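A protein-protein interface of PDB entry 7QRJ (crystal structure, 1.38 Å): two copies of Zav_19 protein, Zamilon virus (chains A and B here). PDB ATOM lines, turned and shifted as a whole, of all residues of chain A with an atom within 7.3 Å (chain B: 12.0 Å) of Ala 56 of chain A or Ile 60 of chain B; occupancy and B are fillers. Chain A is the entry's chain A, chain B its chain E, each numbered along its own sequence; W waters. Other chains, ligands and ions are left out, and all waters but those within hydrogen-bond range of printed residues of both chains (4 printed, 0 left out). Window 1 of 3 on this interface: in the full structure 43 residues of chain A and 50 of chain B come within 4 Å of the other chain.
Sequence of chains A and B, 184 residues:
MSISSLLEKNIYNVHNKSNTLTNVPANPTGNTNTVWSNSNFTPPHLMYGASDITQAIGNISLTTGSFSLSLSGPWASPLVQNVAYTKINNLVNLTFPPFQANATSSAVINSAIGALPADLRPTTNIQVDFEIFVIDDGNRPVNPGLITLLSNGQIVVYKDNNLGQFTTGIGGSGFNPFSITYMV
The side-chain amide nitrogen (ND2) of Asn 59 of chain A sits at hydrogen-bond distance from the backbone carbonyl oxygen (O) of Leu 62 of chain B, at 2.8 Å.
The side-chain hydroxyl (OG1) of Thr 54 of chain B sits at hydrogen-bond distance from the backbone NH (N) of Leu 46 of chain B (2.8 Å). The backbone NH (N) of Ile 53 of chain B is in hydrogen-bond range of the backbone carbonyl oxygen (O) of Leu 46 of chain B, at 2.8 Å.
Among the printed residues, pairs that only touch across the chains: Ile 53 of chain A with Leu 46 of chain B, Ala 56 of chain A with Ile 57 of chain B, Ala 56 of chain A with Ile 60 of chain B, Ile 57 of chain A with Ile 57 of chain B, Ile 60 of chain A with Ile 60 of chain B and Ile 60 of chain A with Leu 62 of chain B.
Printed residues of chain B within 4 Å of Ala 56 of chain A: Ile 57 and Ile 60. Of the printed residues of chain A, Ile 60 of chain B touches Ala 56 (3.995 Å) and Ile 60 (3.96 Å). No residue of chain B comes within 4 Å of Asp 52 of chain A. No residue of chain B comes within 4 Å of Gln 55 of chain A. Of chain B, only Ile 57 comes within 4 Å of Ile 57 of chain A. No residue of chain B comes within 4 Å of Gly 58 of chain A. Asn 59 of chain A touches just one residue of chain B: Leu 62 (2.8 Å). Ile 60 of chain A touches just these residues of chain B: Ile 60 (3.96 Å) and Leu 62 (3.8 Å). Of the printed residues of chain A, Leu 62 of chain B touches Asn 59 and Ile 60. Of the printed residues of chain A, Ile 57 of chain B touches Ala 56 and Ile 57. Printed residues of chain B within 4 Å of Ile 53 of chain A: Leu 46 (3.6 Å). Printed residues of chain A within 4 Å of Leu 46 of chain B: Ile 53. Ser 61 of chain B touches none of the printed residues of chain A. The nearest printed residue of chain B that does not touch Ala 56 of chain A is Gly 58 of chain B (6.0 Å). The nearest printed residue of chain A that does not touch Ile 60 of chain B is Ile 57 of chain A (4.3 Å). The nearest printed residue of chain B that does not touch Ile 53 of chain A is Ile 57 of chain B (4.2 Å).
Of the 22 printed residues of chain B, 4 touch a printed residue of chain A. Printed residues of chain B that touch a printed residue of chain A: Leu 46, Ile 57, Ile 60 and Leu 62. Hydrophobic or aromatic side chains of chain B that line the printed part of chain A: Leu 46, Ile 57, Ile 60 and Leu 62. Along chain B the printed residues that touch a printed residue of chain A span positions 46 to 62. Among the printed residues, 7 pairs touch across the chains. Among the printed residues, no Asp or Glu carboxylate lies within 4 Å of a Lys or Arg side-chain nitrogen of the other chain.
Ala 56 of chain A touches Ile 57 of chain B, but with the chains exchanged Ile 57 of chain A does not touch Ala 56 of chain B (7.3 Å). Ala 56 of chain A touches Ile 60 of chain B, but with the chains exchanged Ile 60 of chain A does not touch Ala 56 of chain B (7.8 Å). Ile 57 of chain B touches its own counterpart, Ile 57 of chain A. Ile 60 of chain A touches its own counterpart, Ile 60 of chain B. Positions printed for both chains: 45, 52, 53, 54, 55, 56, 57, 58, 59, 60 and 61. Of the 7 pairs that touch across the chains among the printed residues, 2 have their exchanged pair printed and touching as well.
Water W1 lies within hydrogen-bond range of the backbone carbonyl oxygen of Ala 56 of chain A (2.7 Å), the backbone carbonyl oxygen of Ile 60 of chain B (2.8 Å) and the side-chain amide nitrogen of Asn 59 of chain A (3.1 Å). Water W4 lies within hydrogen-bond range of OD1 of Asn 59 of chain A and O of Leu 62 of chain B. Water W3 lies within hydrogen-bond range of the side-chain hydroxyl of Ser 51 of chain A (2.9 Å) and the side-chain hydroxyl of Thr 54 of chain B (2.9 Å). Water W2 lies within hydrogen-bond range of the backbone NH (N) of Leu 62 of chain B (3.0 Å) and the side-chain amide nitrogen (ND2) of Asn 59 of chain A (3.5 Å).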
ATOM      1  N   HIS A  45      21.237  20.204  19.983  1.00  0.00           N
ATOM      2  CA  HIS A  45      21.514  19.498  18.733  1.00  0.00           C
ATOM      3  C   HIS A  45      21.988  18.072  18.985  1.00  0.00           C
ATOM      4  O   HIS A  45      22.870  17.837  19.818  1.00  0.00           O
ATOM      5  CB  HIS A  45      22.563  20.229  17.899  1.00  0.00           C
ATOM      6  CG  HIS A  45      22.044  21.453  17.218  1.00  0.00           C
ATOM      7  ND1 HIS A  45      22.740  22.098  16.218  1.00  0.00           N
ATOM      8  CD2 HIS A  45      20.891  22.146  17.382  1.00  0.00           C
ATOM      9  CE1 HIS A  45      22.032  23.127  15.785  1.00  0.00           C
ATOM     10  NE2 HIS A  45      20.908  23.182  16.479  1.00  0.00           N
ATOM     11  N   SER A  51      29.766  15.323  14.159  1.00  0.00           N
ATOM     12  CA  SER A  51      28.720  15.499  13.157  1.00  0.00           C
ATOM     13  C   SER A  51      27.447  16.004  13.824  1.00  0.00           C
ATOM     14  O   SER A  51      26.875  15.316  14.679  1.00  0.00           O
ATOM     15  CB  SER A  51      28.452  14.156  12.483  1.00  0.00           C
ATOM     16  OG  SER A  51      27.396  14.245  11.548  1.00  0.00           O
ATOM     17  N   ASP A  52      26.988  17.187  13.414  1.00  0.00           N
ATOM     18  CA  ASP A  52      25.789  17.816  13.966  1.00  0.00           C
ATOM     19  C   ASP A  52      24.591  17.468  13.082  1.00  0.00           C
ATOM     20  O   ASP A  52      24.360  18.083  12.037  1.00  0.00           O
ATOM     21  CB  ASP A  52      25.998  19.320  14.098  1.00  0.00           C
ATOM     22  CG  ASP A  52      24.858  20.003  14.826  1.00  0.00           C
ATOM     23  OD1 ASP A  52      23.732  19.448  14.850  1.00  0.00           O
ATOM     24  OD2 ASP A  52      25.079  21.116  15.351  1.00  0.00           O
ATOM     25  N   ILE A  53      23.823  16.474  13.524  1.00  0.00           N
ATOM     26  CA  ILE A  53      22.688  15.983  12.746  1.00  0.00           C
ATOM     27  C   ILE A  53      21.592  17.042  12.677  1.00  0.00           C
ATOM     28  O   ILE A  53      21.046  17.326  11.605  1.00  0.00           O
ATOM     29  CB  ILE A  53      22.177  14.667  13.353  1.00  0.00           C
ATOM     30  CG1 ILE A  53      23.254  13.587  13.223  1.00  0.00           C
ATOM     31  CG2 ILE A  53      20.876  14.236  12.686  1.00  0.00           C
ATOM     32  CD1 ILE A  53      23.043  12.401  14.119  1.00  0.00           C
ATOM     33  N   THR A  54      21.260  17.644  13.822  1.00  0.00           N
ATOM     34  CA  THR A  54      20.202  18.654  13.866  1.00  0.00           C
ATOM     35  C   THR A  54      20.517  19.845  12.965  1.00  0.00           C
ATOM     36  O   THR A  54      19.642  20.339  12.239  1.00  0.00           O
ATOM     37  CB  THR A  54      19.998  19.108  15.316  1.00  0.00           C
ATOM     38  OG1 THR A  54      19.668  17.969  16.122  1.00  0.00           O
ATOM     39  CG2 THR A  54      18.888  20.163  15.426  1.00  0.00           C
ATOM     40  N   GLN A  55      21.769  20.318  12.985  1.00  0.00           N
ATOM     41  CA  GLN A  55      22.126  21.469  12.161  1.00  0.00           C
ATOM     42  C   GLN A  55      21.969  21.160  10.678  1.00  0.00           C
ATOM     43  O   GLN A  55      21.470  21.991   9.907  1.00  0.00           O
ATOM     44  CB  GLN A  55      23.563  21.901  12.453  1.00  0.00           C
ATOM     45  CG  GLN A  55      24.047  23.079  11.604  1.00  0.00           C
ATOM     46  CD  GLN A  55      23.424  24.405  11.980  1.00  0.00           C
ATOM     47  OE1 GLN A  55      23.161  24.677  13.149  1.00  0.00           O
ATOM     48  NE2 GLN A  55      23.220  25.258  10.986  1.00  0.00           N
ATOM     49  N   ALA A  56      22.411  19.977  10.254  1.00  0.00           N
ATOM     50  CA  ALA A  56      22.357  19.653   8.833  1.00  0.00           C
ATOM     51  C   ALA A  56      20.920  19.597   8.337  1.00  0.00           C
ATOM     52  O   ALA A  56      20.603  20.107   7.257  1.00  0.00           O
ATOM     53  CB  ALA A  56      23.070  18.331   8.575  1.00  0.00           C
ATOM     54  N   ILE A  57      20.024  19.018   9.134  1.00  0.00           N
ATOM     55  CA  ILE A  57      18.629  18.938   8.724  1.00  0.00           C
ATOM     56  C   ILE A  57      17.980  20.319   8.753  1.00  0.00           C
ATOM     57  O   ILE A  57      17.185  20.668   7.871  1.00  0.00           O
ATOM     58  CB  ILE A  57      17.891  17.926   9.610  1.00  0.00           C
ATOM     59  CG1 ILE A  57      18.363  16.509   9.285  1.00  0.00           C
ATOM     60  CG2 ILE A  57      16.403  18.079   9.442  1.00  0.00           C
ATOM     61  CD1 ILE A  57      17.862  15.489  10.255  1.00  0.00           C
ATOM     62  N   GLY A  58      18.320  21.134   9.752  1.00  0.00           N
ATOM     63  CA  GLY A  58      17.739  22.466   9.838  1.00  0.00           C
ATOM     64  C   GLY A  58      18.212  23.413   8.754  1.00  0.00           C
ATOM     65  O   GLY A  58      17.560  24.430   8.501  1.00  0.00           O
ATOM     66  N   ASN A  59      19.334  23.099   8.113  1.00  0.00           N
ATOM     67  CA  ASN A  59      19.947  23.955   7.113  1.00  0.00           C
ATOM     68  C   ASN A  59      19.276  23.844   5.752  1.00  0.00           C
ATOM     69  O   ASN A  59      19.534  24.682   4.883  1.00  0.00           O
ATOM     70  CB  ASN A  59      21.420  23.575   7.006  1.00  0.00           C
ATOM     71  CG  ASN A  59      22.180  24.418   6.023  1.00  0.00           C
ATOM     72  OD1 ASN A  59      22.271  25.636   6.168  1.00  0.00           O
ATOM     73  ND2 ASN A  59      22.774  23.767   5.034  1.00  0.00           N
ATOM     74  N   ILE A  60      18.412  22.852   5.548  1.00  0.00           N
ATOM     75  CA  ILE A  60      17.740  22.652   4.272  1.00  0.00           C
ATOM     76  C   ILE A  60      16.242  22.537   4.532  1.00  0.00           C
ATOM     77  O   ILE A  60      15.815  21.774   5.406  1.00  0.00           O
ATOM     78  CB  ILE A  60      18.313  21.444   3.492  1.00  0.00           C
ATOM     79  CG1 ILE A  60      17.594  21.255   2.147  1.00  0.00           C
ATOM     80  CG2 ILE A  60      18.278  20.167   4.323  1.00  0.00           C
ATOM     81  CD1 ILE A  60      18.301  20.275   1.208  1.00  0.00           C
ATOM     82  N   SER A  61      15.452  23.334   3.808  1.00  0.00           N
ATOM     83  CA  SER A  61      14.001  23.430   4.007  1.00  0.00           C
ATOM     84  C   SER A  61      13.296  23.215   2.670  1.00  0.00           C
ATOM     85  O   SER A  61      13.227  24.136   1.846  1.00  0.00           O
ATOM     86  CB  SER A  61      13.612  24.785   4.597  1.00  0.00           C
ATOM     87  OG  SER A  61      14.370  25.106   5.751  1.00  0.00           O
ATOM     88  N   HIS B  45      29.730   5.574  10.451  1.00  0.00           N
ATOM     89  CA  HIS B  45      28.414   6.132  10.147  1.00  0.00           C
ATOM     90  C   HIS B  45      27.373   5.695  11.169  1.00  0.00           C
ATOM     91  O   HIS B  45      27.268   4.504  11.485  1.00  0.00           O
ATOM     92  CB  HIS B  45      27.941   5.711   8.759  1.00  0.00           C
ATOM     93  CG  HIS B  45      28.661   6.399   7.646  1.00  0.00           C
ATOM     94  ND1 HIS B  45      28.223   6.357   6.340  1.00  0.00           N
ATOM     95  CD2 HIS B  45      29.772   7.174   7.646  1.00  0.00           C
ATOM     96  CE1 HIS B  45      29.043   7.062   5.580  1.00  0.00           C
ATOM     97  NE2 HIS B  45      29.991   7.568   6.349  1.00  0.00           N
ATOM     98  N   LEU B  46      26.582   6.658  11.646  1.00  0.00           N
ATOM     99  CA  LEU B  46      25.449   6.348  12.509  1.00  0.00           C
ATOM    100  C   LEU B  46      24.328   5.716  11.690  1.00  0.00           C
ATOM    101  O   LEU B  46      23.933   6.248  10.646  1.00  0.00           O
ATOM    102  CB  LEU B  46      24.945   7.630  13.174  1.00  0.00           C
ATOM    103  CG  LEU B  46      23.757   7.447  14.118  1.00  0.00           C
ATOM    104  CD1 LEU B  46      24.152   6.609  15.322  1.00  0.00           C
ATOM    105  CD2 LEU B  46      23.221   8.807  14.550  1.00  0.00           C
ATOM    106  N   ASP B  52      21.288   4.793   6.837  1.00  0.00           N
ATOM    107  CA  ASP B  52      22.577   5.419   7.135  1.00  0.00           C
ATOM    108  C   ASP B  52      22.332   6.905   7.374  1.00  0.00           C
ATOM    109  O   ASP B  52      22.178   7.684   6.427  1.00  0.00           O
ATOM    110  CB  ASP B  52      23.563   5.156   5.999  1.00  0.00           C
ATOM    111  CG  ASP B  52      24.975   5.608   6.323  1.00  0.00           C
ATOM    112  OD1 ASP B  52      25.137   6.507   7.178  1.00  0.00           O
ATOM    113  OD2 ASP B  52      25.920   5.062   5.710  1.00  0.00           O
ATOM    114  N   ILE B  53      22.275   7.290   8.652  1.00  0.00           N
ATOM    115  CA  ILE B  53      21.992   8.676   9.018  1.00  0.00           C
ATOM    116  C   ILE B  53      23.148   9.582   8.610  1.00  0.00           C
ATOM    117  O   ILE B  53      22.942  10.667   8.051  1.00  0.00           O
ATOM    118  CB  ILE B  53      21.703   8.783  10.528  1.00  0.00           C
ATOM    119  CG1 ILE B  53      20.558   7.850  10.953  1.00  0.00           C
ATOM    120  CG2 ILE B  53      21.387  10.227  10.900  1.00  0.00           C
ATOM    121  CD1 ILE B  53      19.246   8.062  10.232  1.00  0.00           C
ATOM    122  N   THR B  54      24.381   9.156   8.890  1.00  0.00           N
ATOM    123  CA  THR B  54      25.540   9.985   8.577  1.00  0.00           C
ATOM    124  C   THR B  54      25.654  10.238   7.083  1.00  0.00           C
ATOM    125  O   THR B  54      25.904  11.373   6.659  1.00  0.00           O
ATOM    126  CB  THR B  54      26.808   9.320   9.104  1.00  0.00           C
ATOM    127  OG1 THR B  54      26.730   9.249  10.530  1.00  0.00           O
ATOM    128  CG2 THR B  54      28.045  10.119   8.703  1.00  0.00           C
ATOM    129  N   GLN B  55      25.466   9.198   6.262  1.00  0.00           N
ATOM    130  CA  GLN B  55      25.580   9.420   4.828  1.00  0.00           C
ATOM    131  C   GLN B  55      24.469  10.336   4.327  1.00  0.00           C
ATOM    132  O   GLN B  55      24.718  11.230   3.512  1.00  0.00           O
ATOM    133  CB  GLN B  55      25.586   8.098   4.073  1.00  0.00           C
ATOM    134  CG  GLN B  55      25.635   8.273   2.557  1.00  0.00           C
ATOM    135  CD  GLN B  55      27.055   8.259   2.024  1.00  0.00           C
ATOM    136  OE1 GLN B  55      27.460   9.148   1.278  1.00  0.00           O
ATOM    137  NE2 GLN B  55      27.825   7.242   2.412  1.00  0.00           N
ATOM    138  N   ALA B  56      23.242  10.147   4.820  1.00  0.00           N
ATOM    139  CA  ALA B  56      22.141  11.010   4.397  1.00  0.00           C
ATOM    140  C   ALA B  56      22.406  12.463   4.764  1.00  0.00           C
ATOM    141  O   ALA B  56      22.158  13.366   3.959  1.00  0.00           O
ATOM    142  CB  ALA B  56      20.827  10.535   5.015  1.00  0.00           C
ATOM    143  N   ILE B  57      22.888  12.699   5.990  1.00  0.00           N
ATOM    144  CA  ILE B  57      23.229  14.044   6.460  1.00  0.00           C
ATOM    145  C   ILE B  57      24.306  14.668   5.584  1.00  0.00           C
ATOM    146  O   ILE B  57      24.227  15.846   5.214  1.00  0.00           O
ATOM    147  CB  ILE B  57      23.670  13.967   7.940  1.00  0.00           C
ATOM    148  CG1 ILE B  57      22.458  13.801   8.857  1.00  0.00           C
ATOM    149  CG2 ILE B  57      24.567  15.143   8.343  1.00  0.00           C
ATOM    150  CD1 ILE B  57      21.278  14.591   8.443  1.00  0.00           C
ATOM    151  N   GLY B  58      25.340  13.896   5.258  1.00  0.00           N
ATOM    152  CA  GLY B  58      26.395  14.424   4.413  1.00  0.00           C
ATOM    153  C   GLY B  58      25.901  14.780   3.028  1.00  0.00           C
ATOM    154  O   GLY B  58      26.394  15.728   2.411  1.00  0.00           O
ATOM    155  N   ASN B  59      24.898  14.053   2.538  1.00  0.00           N
ATOM    156  CA  ASN B  59      24.413  14.227   1.177  1.00  0.00           C
ATOM    157  C   ASN B  59      23.504  15.431   1.013  1.00  0.00           C
ATOM    158  O   ASN B  59      23.238  15.826  -0.126  1.00  0.00           O
ATOM    159  CB  ASN B  59      23.674  12.968   0.721  1.00  0.00           C
ATOM    160  CG  ASN B  59      24.623  11.859   0.308  1.00  0.00           C
ATOM    161  OD1 ASN B  59      25.818  12.085   0.145  1.00  0.00           O
ATOM    162  ND2 ASN B  59      24.094  10.654   0.130  1.00  0.00           N
ATOM    163  N   ILE B  60      23.026  16.023   2.111  1.00  0.00           N
ATOM    164  CA  ILE B  60      22.086  17.138   2.028  1.00  0.00           C
ATOM    165  C   ILE B  60      22.769  18.455   2.378  1.00  0.00           C
ATOM    166  O   ILE B  60      22.106  19.412   2.787  1.00  0.00           O
ATOM    167  CB  ILE B  60      20.822  16.914   2.886  1.00  0.00           C
ATOM    168  CG1 ILE B  60      21.165  16.853   4.377  1.00  0.00           C
ATOM    169  CG2 ILE B  60      20.096  15.643   2.454  1.00  0.00           C
ATOM    170  CD1 ILE B  60      19.946  16.701   5.275  1.00  0.00           C
ATOM    171  N   SER B  61      24.091  18.519   2.222  1.00  0.00           N
ATOM    172  CA  SER B  61      24.805  19.774   2.407  1.00  0.00           C
ATOM    173  C   SER B  61      24.189  20.859   1.533  1.00  0.00           C
ATOM    174  O   SER B  61      23.789  20.610   0.390  1.00  0.00           O
ATOM    175  CB  SER B  61      26.276  19.594   2.033  1.00  0.00           C
ATOM    176  OG  SER B  61      26.410  19.090   0.708  1.00  0.00           O
ATOM    177  N   LEU B  62      24.090  22.068   2.085  1.00  0.00           N
ATOM    178  CA  LEU B  62      23.541  23.194   1.340  1.00  0.00           C
ATOM    179  C   LEU B  62      24.239  24.473   1.768  1.00  0.00           C
ATOM    180  O   LEU B  62      24.358  24.746   2.967  1.00  0.00           O
ATOM    181  CB  LEU B  62      22.021  23.321   1.546  1.00  0.00           C
ATOM    182  CG  LEU B  62      21.237  24.414   0.798  1.00  0.00           C
ATOM    183  CD1 LEU B  62      19.781  24.008   0.637  1.00  0.00           C
ATOM    184  CD2 LEU B  62      21.309  25.771   1.514  1.00  0.00           C
ATOM    185  N   THR B  63      24.675  25.258   0.786  1.00  0.00           N
ATOM    186  CA  THR B  63      25.088  26.632   1.013  1.00  0.00           C
ATOM    187  C   THR B  63      24.319  27.532   0.059  1.00  0.00           C
ATOM    188  O   THR B  63      23.881  27.099  -1.005  1.00  0.00           O
ATOM    189  CB  THR B  63      26.612  26.821   0.851  1.00  0.00           C
ATOM    190  OG1 THR B  63      27.025  26.303  -0.417  1.00  0.00           O
ATOM    191  CG2 THR B  63      27.369  26.100   1.963  1.00  0.00           C
ATOM    192  N   THR B  64      24.127  28.782   0.464  1.00  0.00           N
ATOM    193  CA  THR B  64      23.392  29.731  -0.357  1.00  0.00           C
ATOM    194  C   THR B  64      23.793  31.138   0.052  1.00  0.00           C
ATOM    195  O   THR B  64      24.227  31.368   1.182  1.00  0.00           O
ATOM    196  CB  THR B  64      21.871  29.507  -0.240  1.00  0.00           C
ATOM    197  OG1 THR B  64      21.172  30.314  -1.196  1.00  0.00           O
ATOM    198  CG2 THR B  64      21.376  29.839   1.151  1.00  0.00           C
ATOM    199  N   THR B  86      22.695  28.913  -4.991  1.00  0.00           N
ATOM    200  CA  THR B  86      22.429  27.820  -4.071  1.00  0.00           C
ATOM    201  C   THR B  86      23.271  26.635  -4.517  1.00  0.00           C
ATOM    202  O   THR B  86      23.356  26.358  -5.715  1.00  0.00           O
ATOM    203  CB  THR B  86      20.940  27.420  -4.089  1.00  0.00           C
ATOM    204  OG1 THR B  86      20.133  28.563  -3.788  1.00  0.00           O
ATOM    205  CG2 THR B  86      20.662  26.345  -3.055  1.00  0.00           C
ATOM    206  N   LYS B  87      23.904  25.945  -3.569  1.00  0.00           N
ATOM    207  CA  LYS B  87      24.581  24.689  -3.874  1.00  0.00           C
ATOM    208  C   LYS B  87      24.070  23.624  -2.916  1.00  0.00           C
ATOM    209  O   LYS B  87      24.159  23.792  -1.698  1.00  0.00           O
ATOM    210  CB  LYS B  87      26.109  24.811  -3.796  1.00  0.00           C
ATOM    211  CG  LYS B  87      26.812  23.523  -4.236  1.00  0.00           C
ATOM    212  CD  LYS B  87      28.325  23.669  -4.278  1.00  0.00           C
ATOM    213  CE  LYS B  87      28.976  22.429  -4.882  1.00  0.00           C
ATOM    214  NZ  LYS B  87      30.467  22.506  -4.839  1.00  0.00           N
ATOM    215  N   ILE B  88      23.530  22.539  -3.465  1.00  0.00           N
ATOM    216  CA  ILE B  88      23.006  21.414  -2.691  1.00  0.00           C
ATOM    217  C   ILE B  88      23.758  20.188  -3.169  1.00  0.00           C
ATOM    218  O   ILE B  88      23.613  19.793  -4.329  1.00  0.00           O
ATOM    219  CB  ILE B  88      21.497  21.215  -2.893  1.00  0.00           C
ATOM    220  CG1 ILE B  88      20.720  22.505  -2.650  1.00  0.00           C
ATOM    221  CG2 ILE B  88      20.976  20.092  -2.003  1.00  0.00           C
ATOM    222  CD1 ILE B  88      19.268  22.409  -3.099  1.00  0.00           C
ATOM    223  N   ASN B  89      24.557  19.583  -2.294  1.00  0.00           N
ATOM    224  CA  ASN B  89      25.436  18.507  -2.743  1.00  0.00           C
ATOM    225  C   ASN B  89      26.294  19.040  -3.893  1.00  0.00           C
ATOM    226  O   ASN B  89      27.014  20.022  -3.702  1.00  0.00           O
ATOM    227  CB  ASN B  89      24.641  17.237  -3.099  1.00  0.00           C
ATOM    228  CG  ASN B  89      25.492  15.976  -3.077  1.00  0.00           C
ATOM    229  OD1 ASN B  89      26.445  15.844  -3.837  1.00  0.00           O
ATOM    230  ND2 ASN B  89      25.116  15.024  -2.233  1.00  0.00           N
ATOM    231  N   ASN B  90      26.220  18.448  -5.089  1.00  0.00           N
ATOM    232  CA  ASN B  90      26.989  18.930  -6.234  1.00  0.00           C
ATOM    233  C   ASN B  90      26.183  19.812  -7.185  1.00  0.00           C
ATOM    234  O   ASN B  90      26.695  20.184  -8.249  1.00  0.00           O
ATOM    235  CB  ASN B  90      27.592  17.755  -7.007  1.00  0.00           C
ATOM    236  CG  ASN B  90      28.633  17.010  -6.208  1.00  0.00           C
ATOM    237  OD1 ASN B  90      29.336  17.599  -5.384  1.00  0.00           O
ATOM    238  ND2 ASN B  90      28.730  15.708  -6.434  1.00  0.00           N
ATOM    239  N   LEU B  91      24.937  20.122  -6.844  1.00  0.00           N
ATOM    240  CA  LEU B  91      24.020  20.853  -7.715  1.00  0.00           C
ATOM    241  C   LEU B  91      24.042  22.348  -7.411  1.00  0.00           C
ATOM    242  O   LEU B  91      23.875  22.750  -6.257  1.00  0.00           O
ATOM    243  CB  LEU B  91      22.605  20.307  -7.519  1.00  0.00           C
ATOM    244  CG  LEU B  91      21.495  20.927  -8.368  1.00  0.00           C
ATOM    245  CD1 LEU B  91      21.742  20.705  -9.852  1.00  0.00           C
ATOM    246  CD2 LEU B  91      20.148  20.345  -7.959  1.00  0.00           C
ATOM    247  N   VAL B  92      24.211  23.170  -8.450  1.00  0.00           N
ATOM    248  CA  VAL B  92      24.344  24.621  -8.310  1.00  0.00           C
ATOM    249  C   VAL B  92      23.228  25.328  -9.069  1.00  0.00           C
ATOM    250  O   VAL B  92      22.949  25.003 -10.227  1.00  0.00           O
ATOM    251  CB  VAL B  92      25.706  25.116  -8.829  1.00  0.00           C
ATOM    252  CG1 VAL B  92      25.787  26.648  -8.779  1.00  0.00           C
ATOM    253  CG2 VAL B  92      26.838  24.487  -8.035  1.00  0.00           C
HETATM  254  O   HOH W   1      22.175  20.770   5.194  1.00  0.00           O
HETATM  255  O   HOH W   2      25.905  22.419   4.487  1.00  0.00           O
HETATM  256  O   HOH W   3      25.954  11.785  11.613  1.00  0.00           O
HETATM  257  O   HOH W   4      24.371  26.982   5.162  1.00  0.00           O
